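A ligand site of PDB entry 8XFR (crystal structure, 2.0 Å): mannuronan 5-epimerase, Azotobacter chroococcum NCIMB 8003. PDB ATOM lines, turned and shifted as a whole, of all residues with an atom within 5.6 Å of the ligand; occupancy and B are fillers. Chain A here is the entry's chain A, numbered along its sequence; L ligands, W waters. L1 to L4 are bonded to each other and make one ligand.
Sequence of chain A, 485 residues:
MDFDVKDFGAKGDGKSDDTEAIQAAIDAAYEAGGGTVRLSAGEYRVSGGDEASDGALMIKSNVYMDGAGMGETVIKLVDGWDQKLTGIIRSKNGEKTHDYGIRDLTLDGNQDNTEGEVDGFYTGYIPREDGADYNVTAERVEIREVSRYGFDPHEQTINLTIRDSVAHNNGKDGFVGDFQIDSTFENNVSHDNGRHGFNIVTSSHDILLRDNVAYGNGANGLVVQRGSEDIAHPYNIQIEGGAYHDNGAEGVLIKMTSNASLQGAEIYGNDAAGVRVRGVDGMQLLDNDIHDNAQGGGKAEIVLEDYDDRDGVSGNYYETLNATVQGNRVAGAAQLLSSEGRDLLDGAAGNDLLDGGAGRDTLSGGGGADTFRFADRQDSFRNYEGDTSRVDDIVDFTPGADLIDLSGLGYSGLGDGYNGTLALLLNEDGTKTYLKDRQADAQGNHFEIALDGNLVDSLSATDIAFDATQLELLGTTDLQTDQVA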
ATOM      1  N   GLU A  51     -33.540   6.674   8.298  1.00  0.00           N
ATOM      2  CA  GLU A  51     -32.290   6.501   7.577  1.00  0.00           C
ATOM      3  C   GLU A  51     -31.188   6.038   8.527  1.00  0.00           C
ATOM      4  O   GLU A  51     -31.273   6.211   9.749  1.00  0.00           O
ATOM      5  CB  GLU A  51     -31.883   7.811   6.879  1.00  0.00           C
ATOM      6  CG  GLU A  51     -32.337   7.888   5.425  1.00  0.00           C
ATOM      7  CD  GLU A  51     -32.549   6.501   4.805  1.00  0.00           C
ATOM      8  OE1 GLU A  51     -31.523   5.823   4.515  1.00  0.00           O
ATOM      9  OE2 GLU A  51     -33.721   6.087   4.647  1.00  0.00           O
ATOM     10  N   ALA A  52     -30.180   5.385   7.935  1.00  0.00           N
ATOM     11  CA  ALA A  52     -29.037   4.926   8.713  1.00  0.00           C
ATOM     12  C   ALA A  52     -28.338   6.102   9.392  1.00  0.00           C
ATOM     13  O   ALA A  52     -27.872   5.994  10.527  1.00  0.00           O
ATOM     14  CB  ALA A  52     -28.057   4.171   7.817  1.00  0.00           C
ATOM     15  N   SER A  53     -28.274   7.255   8.705  1.00  0.00           N
ATOM     16  CA  SER A  53     -27.655   8.456   9.243  1.00  0.00           C
ATOM     17  C   SER A  53     -28.444   9.047  10.398  1.00  0.00           C
ATOM     18  O   SER A  53     -27.936   9.934  11.075  1.00  0.00           O
ATOM     19  CB  SER A  53     -27.471   9.496   8.141  1.00  0.00           C
ATOM     20  OG  SER A  53     -28.705  10.004   7.651  1.00  0.00           O
ATOM     21  N   ASP A  54     -29.661   8.591  10.653  1.00  0.00           N
ATOM     22  CA  ASP A  54     -30.362   9.059  11.844  1.00  0.00           C
ATOM     23  C   ASP A  54     -29.811   8.422  13.118  1.00  0.00           C
ATOM     24  O   ASP A  54     -30.089   8.924  14.214  1.00  0.00           O
ATOM     25  CB  ASP A  54     -31.856   8.802  11.730  1.00  0.00           C
ATOM     26  CG  ASP A  54     -32.517   9.653  10.655  1.00  0.00           C
ATOM     27  OD1 ASP A  54     -33.444   9.138   9.981  1.00  0.00           O
ATOM     28  OD2 ASP A  54     -32.109  10.814  10.466  1.00  0.00           O
ATOM     29  N   LYS A  84     -29.629  -0.871   8.687  1.00  0.00           N
ATOM     30  CA  LYS A  84     -28.303  -0.331   8.996  1.00  0.00           C
ATOM     31  C   LYS A  84     -28.474   0.924   9.838  1.00  0.00           C
ATOM     32  O   LYS A  84     -29.319   1.778   9.535  1.00  0.00           O
ATOM     33  CB  LYS A  84     -27.537  -0.038   7.701  1.00  0.00           C
ATOM     34  CG  LYS A  84     -26.157   0.610   7.894  1.00  0.00           C
ATOM     35  CD  LYS A  84     -25.729   1.436   6.652  1.00  0.00           C
ATOM     36  CE  LYS A  84     -24.263   1.188   6.254  1.00  0.00           C
ATOM     37  NZ  LYS A  84     -23.834   2.033   5.091  1.00  0.00           N
ATOM     38  N   THR A  86     -26.186   3.823  11.849  1.00  0.00           N
ATOM     39  CA  THR A  86     -24.842   4.401  11.946  1.00  0.00           C
ATOM     40  C   THR A  86     -24.753   5.281  13.187  1.00  0.00           C
ATOM     41  O   THR A  86     -24.883   6.507  13.139  1.00  0.00           O
ATOM     42  CB  THR A  86     -24.519   5.172  10.667  1.00  0.00           C
ATOM     43  OG1 THR A  86     -24.727   4.317   9.536  1.00  0.00           O
ATOM     44  CG2 THR A  86     -23.066   5.656  10.679  1.00  0.00           C
ATOM     45  N   ARG A  90     -24.918   9.263  18.281  1.00  0.00           N
ATOM     46  CA  ARG A  90     -24.223   9.913  17.187  1.00  0.00           C
ATOM     47  C   ARG A  90     -24.521  11.400  17.175  1.00  0.00           C
ATOM     48  O   ARG A  90     -25.546  11.857  17.698  1.00  0.00           O
ATOM     49  CB  ARG A  90     -24.602   9.288  15.833  1.00  0.00           C
ATOM     50  CG  ARG A  90     -25.907   9.789  15.254  1.00  0.00           C
ATOM     51  CD  ARG A  90     -26.002   9.372  13.796  1.00  0.00           C
ATOM     52  NE  ARG A  90     -25.268  10.290  12.927  1.00  0.00           N
ATOM     53  CZ  ARG A  90     -24.734   9.982  11.748  1.00  0.00           C
ATOM     54  NH1 ARG A  90     -24.778   8.736  11.278  1.00  0.00           N
ATOM     55  NH2 ARG A  90     -24.170  10.933  11.019  1.00  0.00           N
ATOM     56  N   ASN A  93     -24.986  14.461  11.015  1.00  0.00           N
ATOM     57  CA  ASN A  93     -24.283  14.734   9.762  1.00  0.00           C
ATOM     58  C   ASN A  93     -24.535  16.176   9.321  1.00  0.00           C
ATOM     59  O   ASN A  93     -25.671  16.666   9.352  1.00  0.00           O
ATOM     60  CB  ASN A  93     -24.749  13.740   8.690  1.00  0.00           C
ATOM     61  CG  ASN A  93     -24.037  13.917   7.362  1.00  0.00           C
ATOM     62  OD1 ASN A  93     -24.237  14.908   6.677  1.00  0.00           O
ATOM     63  ND2 ASN A  93     -23.231  12.931   6.981  1.00  0.00           N
ATOM     64  N   ASP A 119     -23.184   0.575  14.214  1.00  0.00           N
ATOM     65  CA  ASP A 119     -22.005   1.165  14.842  1.00  0.00           C
ATOM     66  C   ASP A 119     -22.433   1.795  16.152  1.00  0.00           C
ATOM     67  O   ASP A 119     -23.542   2.332  16.250  1.00  0.00           O
ATOM     68  CB  ASP A 119     -21.352   2.185  13.928  1.00  0.00           C
ATOM     69  CG  ASP A 119     -21.132   1.622  12.526  1.00  0.00           C
ATOM     70  OD1 ASP A 119     -20.449   0.579  12.429  1.00  0.00           O
ATOM     71  OD2 ASP A 119     -21.664   2.191  11.536  1.00  0.00           O
ATOM     72  N   TYR A 122     -20.830   7.324  16.867  1.00  0.00           N
ATOM     73  CA  TYR A 122     -20.445   7.884  15.580  1.00  0.00           C
ATOM     74  C   TYR A 122     -20.376   9.400  15.674  1.00  0.00           C
ATOM     75  O   TYR A 122     -21.292  10.031  16.216  1.00  0.00           O
ATOM     76  CB  TYR A 122     -21.443   7.478  14.489  1.00  0.00           C
ATOM     77  CG  TYR A 122     -21.011   7.807  13.095  1.00  0.00           C
ATOM     78  CD1 TYR A 122     -20.281   6.897  12.330  1.00  0.00           C
ATOM     79  CD2 TYR A 122     -21.343   9.027  12.517  1.00  0.00           C
ATOM     80  CE1 TYR A 122     -19.911   7.194  11.028  1.00  0.00           C
ATOM     81  CE2 TYR A 122     -20.960   9.339  11.225  1.00  0.00           C
ATOM     82  CZ  TYR A 122     -20.243   8.416  10.490  1.00  0.00           C
ATOM     83  OH  TYR A 122     -19.881   8.749   9.206  1.00  0.00           O
ATOM     84  N   ILE A 126     -18.995  15.782   7.648  1.00  0.00           N
ATOM     85  CA  ILE A 126     -19.442  15.362   6.313  1.00  0.00           C
ATOM     86  C   ILE A 126     -18.272  14.700   5.601  1.00  0.00           C
ATOM     87  O   ILE A 126     -17.236  15.358   5.385  1.00  0.00           O
ATOM     88  CB  ILE A 126     -19.960  16.518   5.430  1.00  0.00           C
ATOM     89  CG1 ILE A 126     -20.994  17.395   6.120  1.00  0.00           C
ATOM     90  CG2 ILE A 126     -20.608  15.948   4.165  1.00  0.00           C
ATOM     91  CD1 ILE A 126     -21.531  18.471   5.211  1.00  0.00           C
ATOM     92  N   PRO A 127     -18.386  13.442   5.202  1.00  0.00           N
ATOM     93  CA  PRO A 127     -17.295  12.797   4.469  1.00  0.00           C
ATOM     94  C   PRO A 127     -16.824  13.642   3.285  1.00  0.00           C
ATOM     95  O   PRO A 127     -17.630  14.195   2.539  1.00  0.00           O
ATOM     96  CB  PRO A 127     -17.902  11.467   4.018  1.00  0.00           C
ATOM     97  CG  PRO A 127     -19.068  11.202   4.994  1.00  0.00           C
ATOM     98  CD  PRO A 127     -19.470  12.522   5.593  1.00  0.00           C
ATOM     99  N   ARG A 128     -15.507  13.818   3.185  1.00  0.00           N
ATOM    100  CA  ARG A 128     -14.812  14.497   2.099  1.00  0.00           C
ATOM    101  C   ARG A 128     -15.097  15.995   2.027  1.00  0.00           C
ATOM    102  O   ARG A 128     -14.783  16.640   1.026  1.00  0.00           O
ATOM    103  CB  ARG A 128     -15.127  13.851   0.726  1.00  0.00           C
ATOM    104  CG  ARG A 128     -14.549  12.462   0.580  1.00  0.00           C
ATOM    105  CD  ARG A 128     -15.198  11.679  -0.572  1.00  0.00           C
ATOM    106  NE  ARG A 128     -16.312  10.833  -0.135  1.00  0.00           N
ATOM    107  CZ  ARG A 128     -16.259   9.888   0.800  1.00  0.00           C
ATOM    108  NH1 ARG A 128     -15.120   9.546   1.391  1.00  0.00           N
ATOM    109  NH2 ARG A 128     -17.379   9.248   1.135  1.00  0.00           N
ATOM    110  N   ARG A 148     -21.041  -3.941  13.582  1.00  0.00           N
ATOM    111  CA  ARG A 148     -19.798  -3.551  12.909  1.00  0.00           C
ATOM    112  C   ARG A 148     -18.781  -2.843  13.813  1.00  0.00           C
ATOM    113  O   ARG A 148     -18.022  -3.536  14.507  1.00  0.00           O
ATOM    114  CB  ARG A 148     -20.164  -2.643  11.709  1.00  0.00           C
ATOM    115  CG  ARG A 148     -19.102  -2.494  10.620  1.00  0.00           C
ATOM    116  CD  ARG A 148     -19.641  -1.754   9.410  1.00  0.00           C
ATOM    117  NE  ARG A 148     -20.061  -0.394   9.717  1.00  0.00           N
ATOM    118  CZ  ARG A 148     -20.199   0.579   8.812  1.00  0.00           C
ATOM    119  NH1 ARG A 148     -19.979   0.356   7.530  1.00  0.00           N
ATOM    120  NH2 ARG A 148     -20.579   1.796   9.216  1.00  0.00           N
ATOM    121  N   TYR A 149     -18.883  -1.530  14.029  1.00  0.00           N
ATOM    122  CA  TYR A 149     -17.807  -0.759  14.648  1.00  0.00           C
ATOM    123  C   TYR A 149     -18.295  -0.250  15.985  1.00  0.00           C
ATOM    124  O   TYR A 149     -19.337   0.429  16.045  1.00  0.00           O
ATOM    125  CB  TYR A 149     -17.391   0.420  13.777  1.00  0.00           C
ATOM    126  CG  TYR A 149     -16.773   0.090  12.429  1.00  0.00           C
ATOM    127  CD1 TYR A 149     -15.788  -0.884  12.296  1.00  0.00           C
ATOM    128  CD2 TYR A 149     -17.203   0.744  11.273  1.00  0.00           C
ATOM    129  CE1 TYR A 149     -15.212  -1.167  11.046  1.00  0.00           C
ATOM    130  CE2 TYR A 149     -16.642   0.460  10.003  1.00  0.00           C
ATOM    131  CZ  TYR A 149     -15.656  -0.513   9.900  1.00  0.00           C
ATOM    132  OH  TYR A 149     -15.095  -0.810   8.670  1.00  0.00           O
ATOM    133  N   ASP A 152     -16.758   4.546  16.793  1.00  0.00           N
ATOM    134  CA  ASP A 152     -16.560   4.860  15.371  1.00  0.00           C
ATOM    135  C   ASP A 152     -16.536   6.370  15.125  1.00  0.00           C
ATOM    136  O   ASP A 152     -17.221   6.855  14.231  1.00  0.00           O
ATOM    137  CB  ASP A 152     -17.669   4.205  14.546  1.00  0.00           C
ATOM    138  CG  ASP A 152     -17.363   4.148  13.034  1.00  0.00           C
ATOM    139  OD1 ASP A 152     -16.208   4.196  12.612  1.00  0.00           O
ATOM    140  OD2 ASP A 152     -18.322   4.030  12.247  1.00  0.00           O
ATOM    141  N   HIS A 154     -15.645   9.787  13.512  1.00  0.00           N
ATOM    142  CA  HIS A 154     -15.574   9.806  12.058  1.00  0.00           C
ATOM    143  C   HIS A 154     -15.238  11.195  11.536  1.00  0.00           C
ATOM    144  O   HIS A 154     -15.021  12.157  12.291  1.00  0.00           O
ATOM    145  CB  HIS A 154     -16.880   9.231  11.500  1.00  0.00           C
ATOM    146  CG  HIS A 154     -16.678   8.341  10.327  1.00  0.00           C
ATOM    147  ND1 HIS A 154     -16.319   7.010  10.439  1.00  0.00           N
ATOM    148  CD2 HIS A 154     -16.774   8.596   9.001  1.00  0.00           C
ATOM    149  CE1 HIS A 154     -16.196   6.485   9.236  1.00  0.00           C
ATOM    150  NE2 HIS A 154     -16.475   7.426   8.344  1.00  0.00           N
ATOM    151  N   GLU A 155     -15.153  11.291  10.207  1.00  0.00           N
ATOM    152  CA  GLU A 155     -14.516  12.424   9.527  1.00  0.00           C
ATOM    153  C   GLU A 155     -15.366  13.684   9.632  1.00  0.00           C
ATOM    154  O   GLU A 155     -16.576  13.609   9.486  1.00  0.00           O
ATOM    155  CB  GLU A 155     -14.300  12.041   8.055  1.00  0.00           C
ATOM    156  CG  GLU A 155     -13.856  13.192   7.154  1.00  0.00           C
ATOM    157  CD  GLU A 155     -13.682  12.752   5.696  1.00  0.00           C
ATOM    158  OE1 GLU A 155     -14.010  11.593   5.393  1.00  0.00           O
ATOM    159  OE2 GLU A 155     -13.215  13.582   4.874  1.00  0.00           O
ATOM    160  N   ASP A 178     -11.446   7.504  12.477  1.00  0.00           N
ATOM    161  CA  ASP A 178     -11.523   7.803  11.048  1.00  0.00           C
ATOM    162  C   ASP A 178     -11.427   9.320  10.891  1.00  0.00           C
ATOM    163  O   ASP A 178     -12.361  10.026  11.269  1.00  0.00           O
ATOM    164  CB  ASP A 178     -12.823   7.248  10.459  1.00  0.00           C
ATOM    165  CG  ASP A 178     -12.986   7.586   8.989  1.00  0.00           C
ATOM    166  OD1 ASP A 178     -13.413   8.721   8.707  1.00  0.00           O
ATOM    167  OD2 ASP A 178     -12.690   6.736   8.113  1.00  0.00           O
ATOM    168  N   THR A 202      -7.861   6.864   7.457  1.00  0.00           N
ATOM    169  CA  THR A 202      -8.462   8.014   6.766  1.00  0.00           C
ATOM    170  C   THR A 202      -7.867   9.332   7.267  1.00  0.00           C
ATOM    171  O   THR A 202      -8.555  10.163   7.856  1.00  0.00           O
ATOM    172  CB  THR A 202      -9.989   8.026   6.907  1.00  0.00           C
ATOM    173  OG1 THR A 202     -10.503   6.700   6.626  1.00  0.00           O
ATOM    174  CG2 THR A 202     -10.674   9.061   5.972  1.00  0.00           C
ATOM    175  N   SER A 228      -8.444   2.399   2.066  1.00  0.00           N
ATOM    176  CA  SER A 228      -8.578   1.887   0.714  1.00  0.00           C
ATOM    177  C   SER A 228      -8.671   2.972  -0.349  1.00  0.00           C
ATOM    178  O   SER A 228      -8.702   2.649  -1.542  1.00  0.00           O
ATOM    179  CB  SER A 228      -9.793   0.953   0.646  1.00  0.00           C
ATOM    180  OG  SER A 228     -10.974   1.646   1.017  1.00  0.00           O
ATOM    181  N   GLU A 229      -8.685   4.239   0.010  1.00  0.00           N
ATOM    182  CA  GLU A 229      -8.819   5.285  -0.990  1.00  0.00           C
ATOM    183  C   GLU A 229      -7.531   6.082  -1.115  1.00  0.00           C
ATOM    184  O   GLU A 229      -6.682   6.105  -0.211  1.00  0.00           O
ATOM    185  CB  GLU A 229      -9.991   6.189  -0.641  1.00  0.00           C
ATOM    186  CG  GLU A 229     -11.316   5.544  -1.055  1.00  0.00           C
ATOM    187  CD  GLU A 229     -12.459   6.025  -0.182  1.00  0.00           C
ATOM    188  OE1 GLU A 229     -13.282   5.163   0.234  1.00  0.00           O
ATOM    189  OE2 GLU A 229     -12.515   7.243   0.090  1.00  0.00           O
ATOM    190  N   ILE A 231      -6.056   8.968  -0.599  1.00  0.00           N
ATOM    191  CA  ILE A 231      -6.186  10.207   0.183  1.00  0.00           C
ATOM    192  C   ILE A 231      -4.910  10.398   0.993  1.00  0.00           C
ATOM    193  O   ILE A 231      -4.066   9.502   1.058  1.00  0.00           O
ATOM    194  CB  ILE A 231      -7.429  10.207   1.114  1.00  0.00           C
ATOM    195  CG1 ILE A 231      -7.433   8.983   2.025  1.00  0.00           C
ATOM    196  CG2 ILE A 231      -8.747  10.261   0.290  1.00  0.00           C
ATOM    197  CD1 ILE A 231      -8.548   8.975   3.006  1.00  0.00           C
HETATM  198  C1  LIG L   1     -29.326  13.800   4.155  1.00  0.00           C
HETATM  199  C2  LIG L   1     -28.875  13.236   5.495  1.00  0.00           C
HETATM  200  O1  LIG L   1     -29.607  12.030   5.800  1.00  0.00           O
HETATM  201  C3  LIG L   1     -27.431  12.897   5.494  1.00  0.00           C
HETATM  202  O2  LIG L   1     -27.141  12.201   6.723  1.00  0.00           O
HETATM  203  C4  LIG L   1     -27.065  11.992   4.360  1.00  0.00           C
HETATM  204  O3  LIG L   1     -25.643  11.900   4.234  1.00  0.00           O
HETATM  205  C5  LIG L   1     -27.558  12.527   3.021  1.00  0.00           C
HETATM  206  O4  LIG L   1     -28.994  12.845   3.035  1.00  0.00           O
HETATM  207  C6  LIG L   1     -27.244  11.457   2.008  1.00  0.00           C
HETATM  208  O5  LIG L   1     -27.658  10.273   2.179  1.00  0.00           O
HETATM  209  O6  LIG L   1     -26.532  11.765   1.003  1.00  0.00           O
HETATM  210  O7  LIG L   1     -30.669  14.045   4.191  1.00  0.00           O
HETATM  211  C1  LG2 L   2     -25.176  10.591   4.555  1.00  0.00           C
HETATM  212  C2  LG2 L   2     -23.918  10.351   3.758  1.00  0.00           C
HETATM  213  O1  LG2 L   2     -23.060  11.497   3.977  1.00  0.00           O
HETATM  214  C3  LG2 L   2     -23.197   9.110   4.163  1.00  0.00           C
HETATM  215  O2  LG2 L   2     -21.889   9.177   3.518  1.00  0.00           O
HETATM  216  C4  LG2 L   2     -23.010   8.944   5.654  1.00  0.00           C
HETATM  217  O3  LG2 L   2     -22.620   7.612   5.987  1.00  0.00           O
HETATM  218  C5  LG2 L   2     -24.317   9.159   6.413  1.00  0.00           C
HETATM  219  O4  LG2 L   2     -24.974  10.424   6.026  1.00  0.00           O
HETATM  220  C6  LG2 L   2     -24.014   9.172   7.882  1.00  0.00           C
HETATM  221  O5  LG2 L   2     -23.490  10.199   8.391  1.00  0.00           O
HETATM  222  O6  LG2 L   2     -24.293   8.156   8.583  1.00  0.00           O
HETATM  223  C1  LG3 L   3     -21.216   7.548   6.230  1.00  0.00           C
HETATM  224  C2  LG3 L   3     -20.936   6.218   6.894  1.00  0.00           C
HETATM  225  O1  LG3 L   3     -21.709   5.199   6.247  1.00  0.00           O
HETATM  226  C3  LG3 L   3     -19.479   5.939   6.939  1.00  0.00           C
HETATM  227  O2  LG3 L   3     -19.293   4.672   7.630  1.00  0.00           O
HETATM  228  C4  LG3 L   3     -18.731   6.083   5.643  1.00  0.00           C
HETATM  229  O3  LG3 L   3     -17.346   6.003   5.997  1.00  0.00           O
HETATM  230  C5  LG3 L   3     -19.032   7.465   5.036  1.00  0.00           C
HETATM  231  O4  LG3 L   3     -20.475   7.728   4.942  1.00  0.00           O
HETATM  232  C6  LG3 L   3     -18.498   7.668   3.628  1.00  0.00           C
HETATM  233  O5  LG3 L   3     -19.275   7.542   2.629  1.00  0.00           O
HETATM  234  O6  LG3 L   3     -17.299   8.005   3.419  1.00  0.00           O
HETATM  235  C1  LG4 L   4     -16.530   5.488   4.918  1.00  0.00           C
HETATM  236  C2  LG4 L   4     -15.177   6.253   4.804  1.00  0.00           C
HETATM  237  O1  LG4 L   4     -14.334   6.048   5.951  1.00  0.00           O
HETATM  238  C3  LG4 L   4     -14.406   5.787   3.613  1.00  0.00           C
HETATM  239  O2  LG4 L   4     -13.153   6.563   3.499  1.00  0.00           O
HETATM  240  C4  LG4 L   4     -14.226   4.279   3.677  1.00  0.00           C
HETATM  241  O3  LG4 L   4     -13.609   3.766   2.479  1.00  0.00           O
HETATM  242  C5  LG4 L   4     -15.565   3.547   3.869  1.00  0.00           C
HETATM  243  O4  LG4 L   4     -16.315   4.006   5.051  1.00  0.00           O
HETATM  244  C6  LG4 L   4     -15.315   2.073   3.991  1.00  0.00           C
HETATM  245  O5  LG4 L   4     -15.911   1.277   3.210  1.00  0.00           O
HETATM  246  O6  LG4 L   4     -14.504   1.647   4.870  1.00  0.00           O
HETATM  247  O   HOH W   1     -14.324   9.133   6.126  1.00  0.00           O
HETATM  248  O   HOH W   2     -18.065   3.827   9.672  1.00  0.00           O
HETATM  249  O   HOH W   3     -30.653  11.861   8.542  1.00  0.00           O
HETATM  250  O   HOH W   4     -10.814   5.728   4.099  1.00  0.00           O
HETATM  251  O   HOH W   5     -24.280   5.679   7.251  1.00  0.00           O
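NZ of Lys 84 touches O1 of LG3 L3, at 3.98 Å.
Thr 86 touches the ligand.
Tyr 122 touches the ligand.
CB of Pro 127 touches O6 of LG3 L3, 3.6 Å away.
NH2 of Arg 148 touches O2 of LG3 L3 (3.5 Å).
OG1 of Thr 202 touches O1 of LG4 L4 (3.9 Å).
OG of Ser 228 touches O3 of LG4 L4, at 3.7 Å.
Hydrophobic or aromatic side chains within 4 Å of the ligand: Tyr 122, Pro 127 and His 154.
14 residues have an atom within 4 Å of the ligand: Ser 53, Lys 84, Thr 86, Arg 90, Asn 93, Tyr 122, Pro 127, Arg 128, Arg 148, His 154, Asp 178, Thr 202, Ser 228 and Glu 229.
The nearest printed residue that does not touch the ligand is Tyr 149 (4.6 Å).
An oxygen (O1) of LG4 L4 sits at hydrogen-bond distance from the side-chain carboxylate (OD2) of Asp 178, at 2.8 Å.
An oxygen (O3) of LG4 L4 lies within hydrogen-bond range of the side-chain carboxylate (OE1) of Glu 229.
The guanidinium group of Arg 128 lies within salt-bridge range of an oxygen (O6) of LG3 L3 (2.6 Å).
O6 of LG2 L2 is in salt-bridge range of NH1 of Arg 90.
A ring nitrogen (NE2) of His 154 is in hydrogen-bond range of an oxygen (O3) of LG3 L3 (2.9 Å).
O5 of LG2 L2 lies within hydrogen-bond range of ND2 of Asn 93 (3.1 Å).
An oxygen (O2) of LIG L1 lies within hydrogen-bond range of the side-chain hydroxyl of Ser 53, 2.9 Å away.
Water W2 lies within hydrogen-bond range of O2 of LG3 L3 (2.5 Å), OD2 of Asp 152 (2.6 Å) and NH2 of Arg 148 (3.3 Å).
Water W4 lies within hydrogen-bond range of O2 of LG4 L4 (2.6 Å) and OG1 of Thr 202 (2.7 Å).
Water W5 lies within hydrogen-bond range of OG1 of Thr 86 (2.7 Å) and O1 of LG3 L3 (2.8 Å).
Water W3 lies within hydrogen-bond range of OD2 of Asp 54, OG of Ser 53 and O1 of LIG L1.
Water W1 lies within hydrogen-bond range of OE1 of Glu 155 (2.6 Å), OD1 of Asp 178 (2.8 Å) and O1 of LG4 L4 (3.1 Å).
NE of Arg 90 is in hydrogen-bond range of O of Ser 53, 3.3 Å away.
O of Thr 86 lies within hydrogen-bond range of NH1 of Arg 90.
The side-chain carboxylate of Asp 178 lies within hydrogen-bond range of the side-chain hydroxyl of Thr 202 (2.6 Å).
The side-chain carboxylate of Asp 119 lies within salt-bridge range of the guanidinium group of Arg 148 (2.6 Å).
A ring nitrogen (NE2) of His 154 lies within hydrogen-bond range of the side-chain carboxylate of Asp 178 (3.3 Å).
The backbone carbonyl oxygen (O) of Asp 178 sits at hydrogen-bond distance from the backbone NH (N) of Glu 155 (3.2 Å).
N of Arg 128 lies within hydrogen-bond range of OE2 of Glu 155.
NH1 of Arg 128 lies within salt-bridge range of OE2 of Glu 229 (3.7 Å).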
